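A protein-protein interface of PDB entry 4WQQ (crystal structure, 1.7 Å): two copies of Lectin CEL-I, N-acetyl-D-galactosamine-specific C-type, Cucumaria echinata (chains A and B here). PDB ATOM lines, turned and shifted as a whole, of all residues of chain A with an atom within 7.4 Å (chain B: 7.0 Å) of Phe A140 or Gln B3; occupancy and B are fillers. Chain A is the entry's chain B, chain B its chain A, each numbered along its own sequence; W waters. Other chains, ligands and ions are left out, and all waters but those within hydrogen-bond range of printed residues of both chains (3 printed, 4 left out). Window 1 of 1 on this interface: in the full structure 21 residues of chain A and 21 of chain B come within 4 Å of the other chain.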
ATOM      1  N   MET A   1      25.635  -2.057   6.786  1.00  0.00           N
ATOM      2  CA  MET A   1      25.578  -3.409   6.157  1.00  0.00           C
ATOM      3  C   MET A   1      25.075  -3.154   4.771  1.00  0.00           C
ATOM      4  O   MET A   1      24.230  -2.305   4.581  1.00  0.00           O
ATOM      5  CB  MET A   1      24.518  -4.308   6.809  1.00  0.00           C
ATOM      6  CG  MET A   1      24.544  -4.428   8.327  1.00  0.00           C
ATOM      7  SD  MET A   1      22.987  -5.191   8.835  1.00  0.00           S
ATOM      8  CE  MET A   1      22.900  -4.874  10.616  1.00  0.00           C
ATOM      9  N   ASN A   2      25.549  -3.907   3.805  1.00  0.00           N
ATOM     10  CA  ASN A   2      24.914  -3.849   2.501  1.00  0.00           C
ATOM     11  C   ASN A   2      25.116  -5.209   1.883  1.00  0.00           C
ATOM     12  O   ASN A   2      25.968  -6.002   2.345  1.00  0.00           O
ATOM     13  CB  ASN A   2      25.550  -2.789   1.629  1.00  0.00           C
ATOM     14  CG  ASN A   2      26.980  -3.132   1.233  1.00  0.00           C
ATOM     15  OD1 ASN A   2      27.238  -3.724   0.196  1.00  0.00           O
ATOM     16  ND2 ASN A   2      27.944  -2.727   2.067  1.00  0.00           N
ATOM     17  N   GLN A   3      24.382  -5.461   0.821  1.00  0.00           N
ATOM     18  CA  GLN A   3      24.545  -6.725   0.130  1.00  0.00           C
ATOM     19  C   GLN A   3      25.026  -6.538  -1.320  1.00  0.00           C
ATOM     20  O   GLN A   3      24.710  -7.359  -2.173  1.00  0.00           O
ATOM     21  CB  GLN A   3      23.228  -7.456   0.156  1.00  0.00           C
ATOM     22  CG  GLN A   3      22.709  -7.682   1.573  1.00  0.00           C
ATOM     23  CD  GLN A   3      21.994  -6.496   2.187  1.00  0.00           C
ATOM     24  OE1 GLN A   3      21.282  -5.768   1.524  1.00  0.00           O
ATOM     25  NE2 GLN A   3      22.137  -6.347   3.475  1.00  0.00           N
ATOM     26  N   CYS A   4      25.812  -5.505  -1.579  1.00  0.00           N
ATOM     27  CA  CYS A   4      26.474  -5.347  -2.873  1.00  0.00           C
ATOM     28  C   CYS A   4      27.659  -6.325  -3.018  1.00  0.00           C
ATOM     29  O   CYS A   4      28.398  -6.611  -2.068  1.00  0.00           O
ATOM     30  CB  CYS A   4      26.959  -3.923  -3.134  1.00  0.00           C
ATOM     31  SG  CYS A   4      25.552  -2.778  -3.337  1.00  0.00           S
ATOM     32  N   PRO A   5      27.846  -6.843  -4.224  1.00  0.00           N
ATOM     33  CA  PRO A   5      29.036  -7.597  -4.576  1.00  0.00           C
ATOM     34  C   PRO A   5      30.284  -6.747  -4.305  1.00  0.00           C
ATOM     35  O   PRO A   5      30.239  -5.465  -4.277  1.00  0.00           O
ATOM     36  CB  PRO A   5      28.866  -7.904  -6.084  1.00  0.00           C
ATOM     37  CG  PRO A   5      27.420  -7.710  -6.317  1.00  0.00           C
ATOM     38  CD  PRO A   5      26.900  -6.674  -5.328  1.00  0.00           C
ATOM     39  N   GLU A   9      29.419  -0.403  -4.820  1.00  0.00           N
ATOM     40  CA  GLU A   9      28.967   0.473  -3.711  1.00  0.00           C
ATOM     41  C   GLU A   9      27.458   0.568  -3.624  1.00  0.00           C
ATOM     42  O   GLU A   9      26.774   0.686  -4.659  1.00  0.00           O
ATOM     43  CB  GLU A   9      29.556   1.864  -3.898  1.00  0.00           C
ATOM     44  CG  GLU A   9      31.031   1.899  -4.239  1.00  0.00           C
ATOM     45  CD  GLU A   9      31.933   1.483  -3.089  1.00  0.00           C
ATOM     46  OE1 GLU A   9      33.129   1.242  -3.358  1.00  0.00           O
ATOM     47  OE2 GLU A   9      31.441   1.384  -1.958  1.00  0.00           O
ATOM     48  N   ALA A  10      26.916   0.559  -2.386  1.00  0.00           N
ATOM     49  CA  ALA A  10      25.501   0.521  -2.143  1.00  0.00           C
ATOM     50  C   ALA A  10      24.906   1.933  -2.054  1.00  0.00           C
ATOM     51  O   ALA A  10      25.483   2.791  -1.402  1.00  0.00           O
ATOM     52  CB  ALA A  10      25.184  -0.246  -0.880  1.00  0.00           C
ATOM     53  N   GLU A  11      23.794   2.175  -2.716  1.00  0.00           N
ATOM     54  CA  GLU A  11      22.990   3.382  -2.454  1.00  0.00           C
ATOM     55  C   GLU A  11      21.555   3.032  -2.779  1.00  0.00           C
ATOM     56  O   GLU A  11      21.286   2.579  -3.850  1.00  0.00           O
ATOM     57  CB  GLU A  11      23.520   4.535  -3.314  1.00  0.00           C
ATOM     58  CG  GLU A  11      22.971   5.857  -2.965  1.00  0.00           C
ATOM     59  CD  GLU A  11      23.084   6.145  -1.461  1.00  0.00           C
ATOM     60  OE1 GLU A  11      24.146   5.884  -0.798  1.00  0.00           O
ATOM     61  OE2 GLU A  11      22.036   6.510  -0.913  1.00  0.00           O
ATOM     62  N   GLY A  12      20.611   3.225  -1.845  1.00  0.00           N
ATOM     63  CA  GLY A  12      19.230   2.805  -2.011  1.00  0.00           C
ATOM     64  C   GLY A  12      19.090   1.332  -2.268  1.00  0.00           C
ATOM     65  O   GLY A  12      19.748   0.503  -1.657  1.00  0.00           O
ATOM     66  N   ASP A  13      18.276   1.035  -3.237  1.00  0.00           N
ATOM     67  CA  ASP A  13      18.077  -0.276  -3.804  1.00  0.00           C
ATOM     68  C   ASP A  13      19.097  -0.758  -4.840  1.00  0.00           C
ATOM     69  O   ASP A  13      18.866  -1.788  -5.435  1.00  0.00           O
ATOM     70  CB  ASP A  13      16.716  -0.234  -4.522  1.00  0.00           C
ATOM     71  CG  ASP A  13      15.583  -0.362  -3.559  1.00  0.00           C
ATOM     72  OD1 ASP A  13      15.835  -0.933  -2.464  1.00  0.00           O
ATOM     73  OD2 ASP A  13      14.463   0.102  -3.874  1.00  0.00           O
ATOM     74  N   HIS A  14      20.168  -0.030  -5.053  1.00  0.00           N
ATOM     75  CA  HIS A  14      21.076  -0.328  -6.139  1.00  0.00           C
ATOM     76  C   HIS A  14      22.487  -0.504  -5.680  1.00  0.00           C
ATOM     77  O   HIS A  14      22.859  -0.072  -4.594  1.00  0.00           O
ATOM     78  CB  HIS A  14      20.980   0.773  -7.204  1.00  0.00           C
ATOM     79  CG  HIS A  14      19.658   0.813  -7.888  1.00  0.00           C
ATOM     80  ND1 HIS A  14      19.301  -0.106  -8.854  1.00  0.00           N
ATOM     81  CD2 HIS A  14      18.580   1.607  -7.710  1.00  0.00           C
ATOM     82  CE1 HIS A  14      18.092   0.175  -9.296  1.00  0.00           C
ATOM     83  NE2 HIS A  14      17.601   1.157  -8.558  1.00  0.00           N
ATOM     84  N   CYS A  15      23.310  -1.081  -6.558  1.00  0.00           N
ATOM     85  CA  CYS A  15      24.785  -1.082  -6.418  1.00  0.00           C
ATOM     86  C   CYS A  15      25.416  -0.361  -7.584  1.00  0.00           C
ATOM     87  O   CYS A  15      24.859  -0.376  -8.678  1.00  0.00           O
ATOM     88  CB  CYS A  15      25.409  -2.495  -6.242  1.00  0.00           C
ATOM     89  SG  CYS A  15      24.583  -3.447  -5.035  1.00  0.00           S
ATOM     90  N   LEU A  40      20.435 -14.771 -10.614  1.00  0.00           N
ATOM     91  CA  LEU A  40      19.876 -13.995  -9.532  1.00  0.00           C
ATOM     92  C   LEU A  40      19.023 -12.834 -10.030  1.00  0.00           C
ATOM     93  O   LEU A  40      18.641 -11.972  -9.228  1.00  0.00           O
ATOM     94  CB  LEU A  40      21.001 -13.516  -8.597  1.00  0.00           C
ATOM     95  CG  LEU A  40      21.649 -14.681  -7.790  1.00  0.00           C
ATOM     96  CD1 LEU A  40      22.857 -14.180  -7.032  1.00  0.00           C
ATOM     97  CD2 LEU A  40      20.690 -15.283  -6.820  1.00  0.00           C
ATOM     98  N   ASN A  41      18.704 -12.808 -11.334  1.00  0.00           N
ATOM     99  CA  ASN A  41      17.919 -11.745 -11.938  1.00  0.00           C
ATOM    100  C   ASN A  41      18.531 -10.354 -11.677  1.00  0.00           C
ATOM    101  O   ASN A  41      17.850  -9.415 -11.444  1.00  0.00           O
ATOM    102  CB  ASN A  41      16.465 -11.824 -11.458  1.00  0.00           C
ATOM    103  CG  ASN A  41      15.840 -13.119 -11.863  1.00  0.00           C
ATOM    104  OD1 ASN A  41      15.895 -13.480 -13.052  1.00  0.00           O
ATOM    105  ND2 ASN A  41      15.373 -13.879 -10.897  1.00  0.00           N
ATOM    106  N   VAL A  42      19.851 -10.287 -11.747  1.00  0.00           N
ATOM    107  CA  VAL A  42      20.579  -9.032 -11.605  1.00  0.00           C
ATOM    108  C   VAL A  42      20.897  -8.527 -12.992  1.00  0.00           C
ATOM    109  O   VAL A  42      21.559  -9.220 -13.791  1.00  0.00           O
ATOM    110  CB  VAL A  42      21.897  -9.188 -10.884  1.00  0.00           C
ATOM    111  CG1 VAL A  42      22.542  -7.837 -10.606  1.00  0.00           C
ATOM    112  CG2 VAL A  42      21.706  -9.914  -9.558  1.00  0.00           C
ATOM    113  N   ARG A  43      20.441  -7.306 -13.267  1.00  0.00           N
ATOM    114  CA  ARG A  43      20.727  -6.678 -14.543  1.00  0.00           C
ATOM    115  C   ARG A  43      21.763  -5.596 -14.256  1.00  0.00           C
ATOM    116  O   ARG A  43      21.516  -4.702 -13.403  1.00  0.00           O
ATOM    117  CB  ARG A  43      19.494  -6.061 -15.148  1.00  0.00           C
ATOM    118  CG  ARG A  43      18.204  -6.861 -15.098  1.00  0.00           C
ATOM    119  CD  ARG A  43      18.309  -8.314 -15.553  1.00  0.00           C
ATOM    120  NE  ARG A  43      17.022  -8.967 -15.298  1.00  0.00           N
ATOM    121  CZ  ARG A  43      16.866 -10.273 -15.280  1.00  0.00           C
ATOM    122  NH1 ARG A  43      17.880 -11.053 -15.523  1.00  0.00           N
ATOM    123  NH2 ARG A  43      15.687 -10.774 -14.979  1.00  0.00           N
ATOM    124  N   LYS A 137      25.669   0.248 -12.912  1.00  0.00           N
ATOM    125  CA  LYS A 137      24.621   0.162 -11.907  1.00  0.00           C
ATOM    126  C   LYS A 137      23.970  -1.194 -11.948  1.00  0.00           C
ATOM    127  O   LYS A 137      23.606  -1.701 -13.025  1.00  0.00           O
ATOM    128  CB  LYS A 137      23.548   1.240 -12.216  1.00  0.00           C
ATOM    129  CG  LYS A 137      22.343   1.326 -11.292  1.00  0.00           C
ATOM    130  CD  LYS A 137      21.404   2.455 -11.730  1.00  0.00           C
ATOM    131  CE  LYS A 137      20.141   2.480 -11.000  1.00  0.00           C
ATOM    132  NZ  LYS A 137      19.308   3.678 -11.284  1.00  0.00           N
ATOM    133  N   LEU A 138      23.795  -1.805 -10.790  1.00  0.00           N
ATOM    134  CA  LEU A 138      23.003  -3.023 -10.684  1.00  0.00           C
ATOM    135  C   LEU A 138      21.540  -2.719 -10.342  1.00  0.00           C
ATOM    136  O   LEU A 138      21.228  -1.987  -9.400  1.00  0.00           O
ATOM    137  CB  LEU A 138      23.531  -3.958  -9.598  1.00  0.00           C
ATOM    138  CG  LEU A 138      25.010  -4.377  -9.788  1.00  0.00           C
ATOM    139  CD1 LEU A 138      25.372  -5.434  -8.709  1.00  0.00           C
ATOM    140  CD2 LEU A 138      25.251  -4.862 -11.196  1.00  0.00           C
ATOM    141  N   THR A 139      20.678  -3.424 -11.033  1.00  0.00           N
ATOM    142  CA  THR A 139      19.263  -3.500 -10.748  1.00  0.00           C
ATOM    143  C   THR A 139      18.841  -4.911 -10.432  1.00  0.00           C
ATOM    144  O   THR A 139      19.054  -5.852 -11.218  1.00  0.00           O
ATOM    145  CB  THR A 139      18.449  -2.897 -11.896  1.00  0.00           C
ATOM    146  OG1 THR A 139      18.852  -1.532 -12.087  1.00  0.00           O
ATOM    147  CG2 THR A 139      17.000  -2.981 -11.564  1.00  0.00           C
ATOM    148  N   PHE A 140      18.188  -5.048  -9.274  1.00  0.00           N
ATOM    149  CA  PHE A 140      17.734  -6.370  -8.821  1.00  0.00           C
ATOM    150  C   PHE A 140      16.286  -6.533  -9.225  1.00  0.00           C
ATOM    151  O   PHE A 140      15.335  -6.043  -8.546  1.00  0.00           O
ATOM    152  CB  PHE A 140      17.921  -6.478  -7.311  1.00  0.00           C
ATOM    153  CG  PHE A 140      19.332  -6.298  -6.915  1.00  0.00           C
ATOM    154  CD1 PHE A 140      20.225  -7.332  -7.075  1.00  0.00           C
ATOM    155  CD2 PHE A 140      19.816  -5.069  -6.532  1.00  0.00           C
ATOM    156  CE1 PHE A 140      21.562  -7.171  -6.796  1.00  0.00           C
ATOM    157  CE2 PHE A 140      21.140  -4.888  -6.252  1.00  0.00           C
ATOM    158  CZ  PHE A 140      22.031  -5.930  -6.358  1.00  0.00           C
ATOM    159  N   GLU A 141      16.120  -7.141 -10.375  1.00  0.00           N
ATOM    160  CA  GLU A 141      14.823  -7.220 -10.993  1.00  0.00           C
ATOM    161  C   GLU A 141      13.977  -8.249 -10.262  1.00  0.00           C
ATOM    162  O   GLU A 141      14.409  -9.345  -9.869  1.00  0.00           O
ATOM    163  CB  GLU A 141      14.910  -7.496 -12.473  1.00  0.00           C
ATOM    164  CG  GLU A 141      13.539  -7.420 -13.126  1.00  0.00           C
ATOM    165  CD  GLU A 141      13.536  -7.544 -14.651  1.00  0.00           C
ATOM    166  OE1 GLU A 141      12.434  -7.393 -15.277  1.00  0.00           O
ATOM    167  OE2 GLU A 141      14.611  -7.725 -15.224  1.00  0.00           O
ATOM    168  OXT GLU A 141      12.768  -7.932 -10.095  1.00  0.00           O
ATOM    169  N   MET B   1      15.464  -0.336   2.526  1.00  0.00           N
ATOM    170  CA  MET B   1      16.000  -0.781   1.219  1.00  0.00           C
ATOM    171  C   MET B   1      17.156  -1.704   1.464  1.00  0.00           C
ATOM    172  O   MET B   1      17.949  -1.496   2.373  1.00  0.00           O
ATOM    173  CB  MET B   1      16.482   0.416   0.371  1.00  0.00           C
ATOM    174  CG  MET B   1      15.416   1.481   0.152  1.00  0.00           C
ATOM    175  SD  MET B   1      15.739   2.533  -1.292  1.00  0.00           S
ATOM    176  CE  MET B   1      14.264   3.559  -1.328  1.00  0.00           C
ATOM    177  N   ASN B   2      17.307  -2.685   0.588  1.00  0.00           N
ATOM    178  CA  ASN B   2      18.488  -3.555   0.599  1.00  0.00           C
ATOM    179  C   ASN B   2      18.902  -3.862  -0.819  1.00  0.00           C
ATOM    180  O   ASN B   2      18.232  -3.421  -1.766  1.00  0.00           O
ATOM    181  CB  ASN B   2      18.199  -4.847   1.373  1.00  0.00           C
ATOM    182  CG  ASN B   2      17.127  -5.700   0.732  1.00  0.00           C
ATOM    183  OD1 ASN B   2      17.250  -6.195  -0.384  1.00  0.00           O
ATOM    184  ND2 ASN B   2      16.031  -5.863   1.463  1.00  0.00           N
ATOM    185  N   GLN B   3      20.007  -4.591  -0.979  1.00  0.00           N
ATOM    186  CA  GLN B   3      20.502  -4.886  -2.304  1.00  0.00           C
ATOM    187  C   GLN B   3      20.444  -6.401  -2.560  1.00  0.00           C
ATOM    188  O   GLN B   3      21.246  -6.905  -3.348  1.00  0.00           O
ATOM    189  CB  GLN B   3      21.911  -4.363  -2.474  1.00  0.00           C
ATOM    190  CG  GLN B   3      22.025  -2.861  -2.230  1.00  0.00           C
ATOM    191  CD  GLN B   3      22.141  -2.540  -0.759  1.00  0.00           C
ATOM    192  OE1 GLN B   3      22.823  -3.252  -0.030  1.00  0.00           O
ATOM    193  NE2 GLN B   3      21.529  -1.421  -0.319  1.00  0.00           N
ATOM    194  N   CYS B   4      19.513  -7.105  -1.904  1.00  0.00           N
ATOM    195  CA  CYS B   4      19.340  -8.563  -2.186  1.00  0.00           C
ATOM    196  C   CYS B   4      18.573  -8.771  -3.514  1.00  0.00           C
ATOM    197  O   CYS B   4      17.683  -8.004  -3.885  1.00  0.00           O
ATOM    198  CB  CYS B   4      18.658  -9.359  -1.072  1.00  0.00           C
ATOM    199  SG  CYS B   4      19.826  -9.516   0.323  1.00  0.00           S
ATOM    200  N   PRO B   5      18.892  -9.839  -4.224  1.00  0.00           N
ATOM    201  CA  PRO B   5      18.015 -10.225  -5.349  1.00  0.00           C
ATOM    202  C   PRO B   5      16.571 -10.464  -4.915  1.00  0.00           C
ATOM    203  O   PRO B   5      16.304 -10.872  -3.777  1.00  0.00           O
ATOM    204  CB  PRO B   5      18.678 -11.504  -5.894  1.00  0.00           C
ATOM    205  CG  PRO B   5      20.119 -11.353  -5.502  1.00  0.00           C
ATOM    206  CD  PRO B   5      20.158 -10.539  -4.198  1.00  0.00           C
ATOM    207  N   THR B   6      15.645 -10.324  -5.875  1.00  0.00           N
ATOM    208  CA  THR B   6      14.290 -10.624  -5.606  1.00  0.00           C
ATOM    209  C   THR B   6      14.107 -12.075  -5.105  1.00  0.00           C
ATOM    210  O   THR B   6      14.719 -12.985  -5.623  1.00  0.00           O
ATOM    211  CB  THR B   6      13.480 -10.379  -6.900  1.00  0.00           C
ATOM    212  OG1 THR B   6      13.617  -8.973  -7.222  1.00  0.00           O
ATOM    213  CG2 THR B   6      12.016 -10.803  -6.682  1.00  0.00           C
ATOM    214  N   ALA B  10      17.398 -10.043   3.112  1.00  0.00           N
ATOM    215  CA  ALA B  10      18.659  -9.477   3.564  1.00  0.00           C
ATOM    216  C   ALA B  10      18.797  -9.598   5.060  1.00  0.00           C
ATOM    217  O   ALA B  10      17.829  -9.339   5.818  1.00  0.00           O
ATOM    218  CB  ALA B  10      18.765  -8.037   3.154  1.00  0.00           C
ATOM    219  N   CYS B  15      22.461 -12.479   1.910  1.00  0.00           N
ATOM    220  CA  CYS B  15      21.112 -12.724   1.538  1.00  0.00           C
ATOM    221  C   CYS B  15      20.806 -14.184   1.745  1.00  0.00           C
ATOM    222  O   CYS B  15      21.715 -15.010   1.664  1.00  0.00           O
ATOM    223  CB  CYS B  15      20.800 -12.340   0.077  1.00  0.00           C
ATOM    224  SG  CYS B  15      21.318 -10.680  -0.391  1.00  0.00           S
ATOM    225  N   LEU B  40      29.845 -11.624 -10.796  1.00  0.00           N
ATOM    226  CA  LEU B  40      29.814 -10.703  -9.637  1.00  0.00           C
ATOM    227  C   LEU B  40      30.502 -11.310  -8.399  1.00  0.00           C
ATOM    228  O   LEU B  40      30.449 -10.728  -7.306  1.00  0.00           O
ATOM    229  CB  LEU B  40      28.378 -10.314  -9.281  1.00  0.00           C
ATOM    230  CG  LEU B  40      27.674  -9.391 -10.302  1.00  0.00           C
ATOM    231  CD1 LEU B  40      26.144  -9.291 -10.058  1.00  0.00           C
ATOM    232  CD2 LEU B  40      28.343  -8.067 -10.372  1.00  0.00           C
ATOM    233  N   LEU B 138      23.714 -16.199   0.138  1.00  0.00           N
ATOM    234  CA  LEU B 138      24.690 -15.538  -0.693  1.00  0.00           C
ATOM    235  C   LEU B 138      25.863 -14.982   0.074  1.00  0.00           C
ATOM    236  O   LEU B 138      25.679 -14.334   1.107  1.00  0.00           O
ATOM    237  CB  LEU B 138      24.021 -14.418  -1.437  1.00  0.00           C
ATOM    238  CG  LEU B 138      22.842 -14.834  -2.303  1.00  0.00           C
ATOM    239  CD1 LEU B 138      22.419 -13.629  -3.060  1.00  0.00           C
ATOM    240  CD2 LEU B 138      23.065 -16.004  -3.284  1.00  0.00           C
ATOM    241  N   PHE B 140      29.250 -12.554  -0.793  1.00  0.00           N
ATOM    242  CA  PHE B 140      29.897 -11.655  -1.738  1.00  0.00           C
ATOM    243  C   PHE B 140      31.353 -11.724  -1.553  1.00  0.00           C
ATOM    244  O   PHE B 140      31.918 -11.085  -0.685  1.00  0.00           O
ATOM    245  CB  PHE B 140      29.326 -10.287  -1.598  1.00  0.00           C
ATOM    246  CG  PHE B 140      27.825 -10.313  -1.696  1.00  0.00           C
ATOM    247  CD1 PHE B 140      27.200 -10.412  -2.911  1.00  0.00           C
ATOM    248  CD2 PHE B 140      27.046 -10.260  -0.561  1.00  0.00           C
ATOM    249  CE1 PHE B 140      25.817 -10.469  -2.970  1.00  0.00           C
ATOM    250  CE2 PHE B 140      25.670 -10.359  -0.619  1.00  0.00           C
ATOM    251  CZ  PHE B 140      25.039 -10.453  -1.815  1.00  0.00           C
HETATM  252  O   HOH W   1      14.902  -3.077  -0.741  1.00  0.00           O
HETATM  253  O   HOH W   2      23.352  -8.468  -4.303  1.00  0.00           O
HETATM  254  O   HOH W   3      14.714  -6.949  -5.453  1.00  0.00           O
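Gln B3 touches its own counterpart, Gln A3.
Gln A3 touches Cys B4, and with the chains exchanged Cys A4 touches Gln B3.
Gln A3 touches Ala B10, and with the chains exchanged Ala A10 touches Gln B3.
Gln A3 touches Phe B140, and with the chains exchanged Phe A140 touches Gln B3.
SG of Cys B15 is disulfide-bonded to SG of Cys B4, at 2.0 Å.
N of Leu A138 lies within hydrogen-bond range of O of Cys A15.
The backbone NH (N) of Ala B10 sits close to the side-chain sulfur (SG) of Cys B4 (3.7 Å).
The side-chain sulfur (SG) of Cys A4 is disulfide-bonded to the side-chain sulfur (SG) of Cys A15 (2.1 Å).
N of Leu B138 lies within hydrogen-bond range of O of Cys B15 (2.8 Å).
The backbone NH (N) of Ala A10 lies close to the side-chain sulfur (SG) of Cys A4, at 3.7 Å.
OE1 of Gln B3 is in hydrogen-bond range of N of Gln A3 (2.8 Å).
The side-chain amide nitrogen (NE2) of Gln B3 is in hydrogen-bond range of the backbone carbonyl oxygen (O) of Gly A12 (2.9 Å).
The side-chain sulfur (SD) of Met B1 is in hydrogen-bond range of the backbone NH (N) of Asp A13, 3.5 Å away.
OG1 of Thr B6 lies within hydrogen-bond range of O of Glu A141, 2.8 Å away.
Of the printed residues of chain B, Asn A2 touches Gln B3.
Of the printed residues of chain B, Cys A4 touches Gln B3 and Phe B140.
Glu A11 touches none of the printed residues of chain B.
Thr A139 touches none of the printed residues of chain B.
Of chain B, only Gln B3, Cys B4 and Thr B6 come within 4 Å of Phe A140.
Printed residues of chain A within 4 Å of Met B1: Gly A12 (3.6 Å) and Asp A13 (3.2 Å).
Of the printed residues of chain A, Asn B2 touches Gln A3 and Asp A13.
Of chain A, only Asn A2, Gln A3, Cys A4, Ala A10, Gly A12, His A14, Cys A15 and Phe A140 come within 4 Å of Gln B3.
Printed residues of chain A within 4 Å of Thr B6: Phe A140 and Glu A141.
The nearest residue of chain B that does not touch Phe A140 is Pro B5 (4.02 Å).
The nearest residue of chain A that does not touch Gln B3 is Asp A13 (4.5 Å).
The nearest printed residue of chain B that does not touch Asp A13 is Gln B3 (4.5 Å).
Of the 11 printed residues of chain B, 10 touch a printed residue of chain A.
Hydrophobic or aromatic side chains of chain B within 4 Å of the printed part of chain A: Met B1, Pro B5, Ala B10, Leu B40 and Phe B140.
Along chain B the printed residues that touch a printed residue of chain A span positions 1 to 140.
Printed residues of chain A that touch a printed residue of chain B: Asn A2, Gln A3, Cys A4, Pro A5, Ala A10, Gly A12, Asp A13, His A14, Cys A15, Leu A40, Val A42, Phe A140 and Glu A141.
Hydrophobic or aromatic side chains of chain A within 4 Å of the printed part of chain B: Pro A5, Ala A10, Leu A40, Val A42 and Phe A140.
Among the printed residues, 24 pairs touch across the chains.
Among the printed residues, no Asp or Glu carboxylate lies within 4 Å of a Lys or Arg side-chain nitrogen of the other chain.
Water W2 bridges O of Gln A3 (2.8 Å) and O of Gln B3 (2.8 Å).
Water W1 lies within hydrogen-bond range of the backbone NH (N) of Asn B2 (2.8 Å) and the side-chain carboxylate (OD1) of Asp A13 (2.9 Å).
Water W3 lies within hydrogen-bond range of OG1 of Thr B6 (2.9 Å) and O of Phe A140 (3.3 Å).
Among the printed residues, pairs that only touch across the chains: Gln A3 with Phe B140 (3.1 Å), Gln A3 with Asn B2 (3.2 Å), Asn A2 with Gln B3 (3.2 Å), Phe A140 with Gln B3 (3.3 Å), Leu A40 with Pro B5 (3.4 Å), Pro A5 with Leu B40 (3.5 Å), Asp A13 with Asn B2 (3.5 Å), Gly A12 with Met B1 (3.6 Å), Gln A3 with Cys B4 (3.6 Å), Phe A140 with Thr B6 (3.6 Å), Cys A4 with Gln B3 (3.7 Å), Gln A3 with Ala B10 (3.7 Å), His A14 with Gln B3 (3.8 Å), Pro A5 with Phe B140 (3.8 Å), Phe A140 with Cys B4 (3.8 Å), Cys A4 with Phe B140 (3.8 Å), Gln A3 with Cys B15 (3.8 Å), Ala A10 with Gln B3 (3.8 Å), Cys A15 with Gln B3 (3.8 Å) and Val A42 with Leu B40 (3.9 Å).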
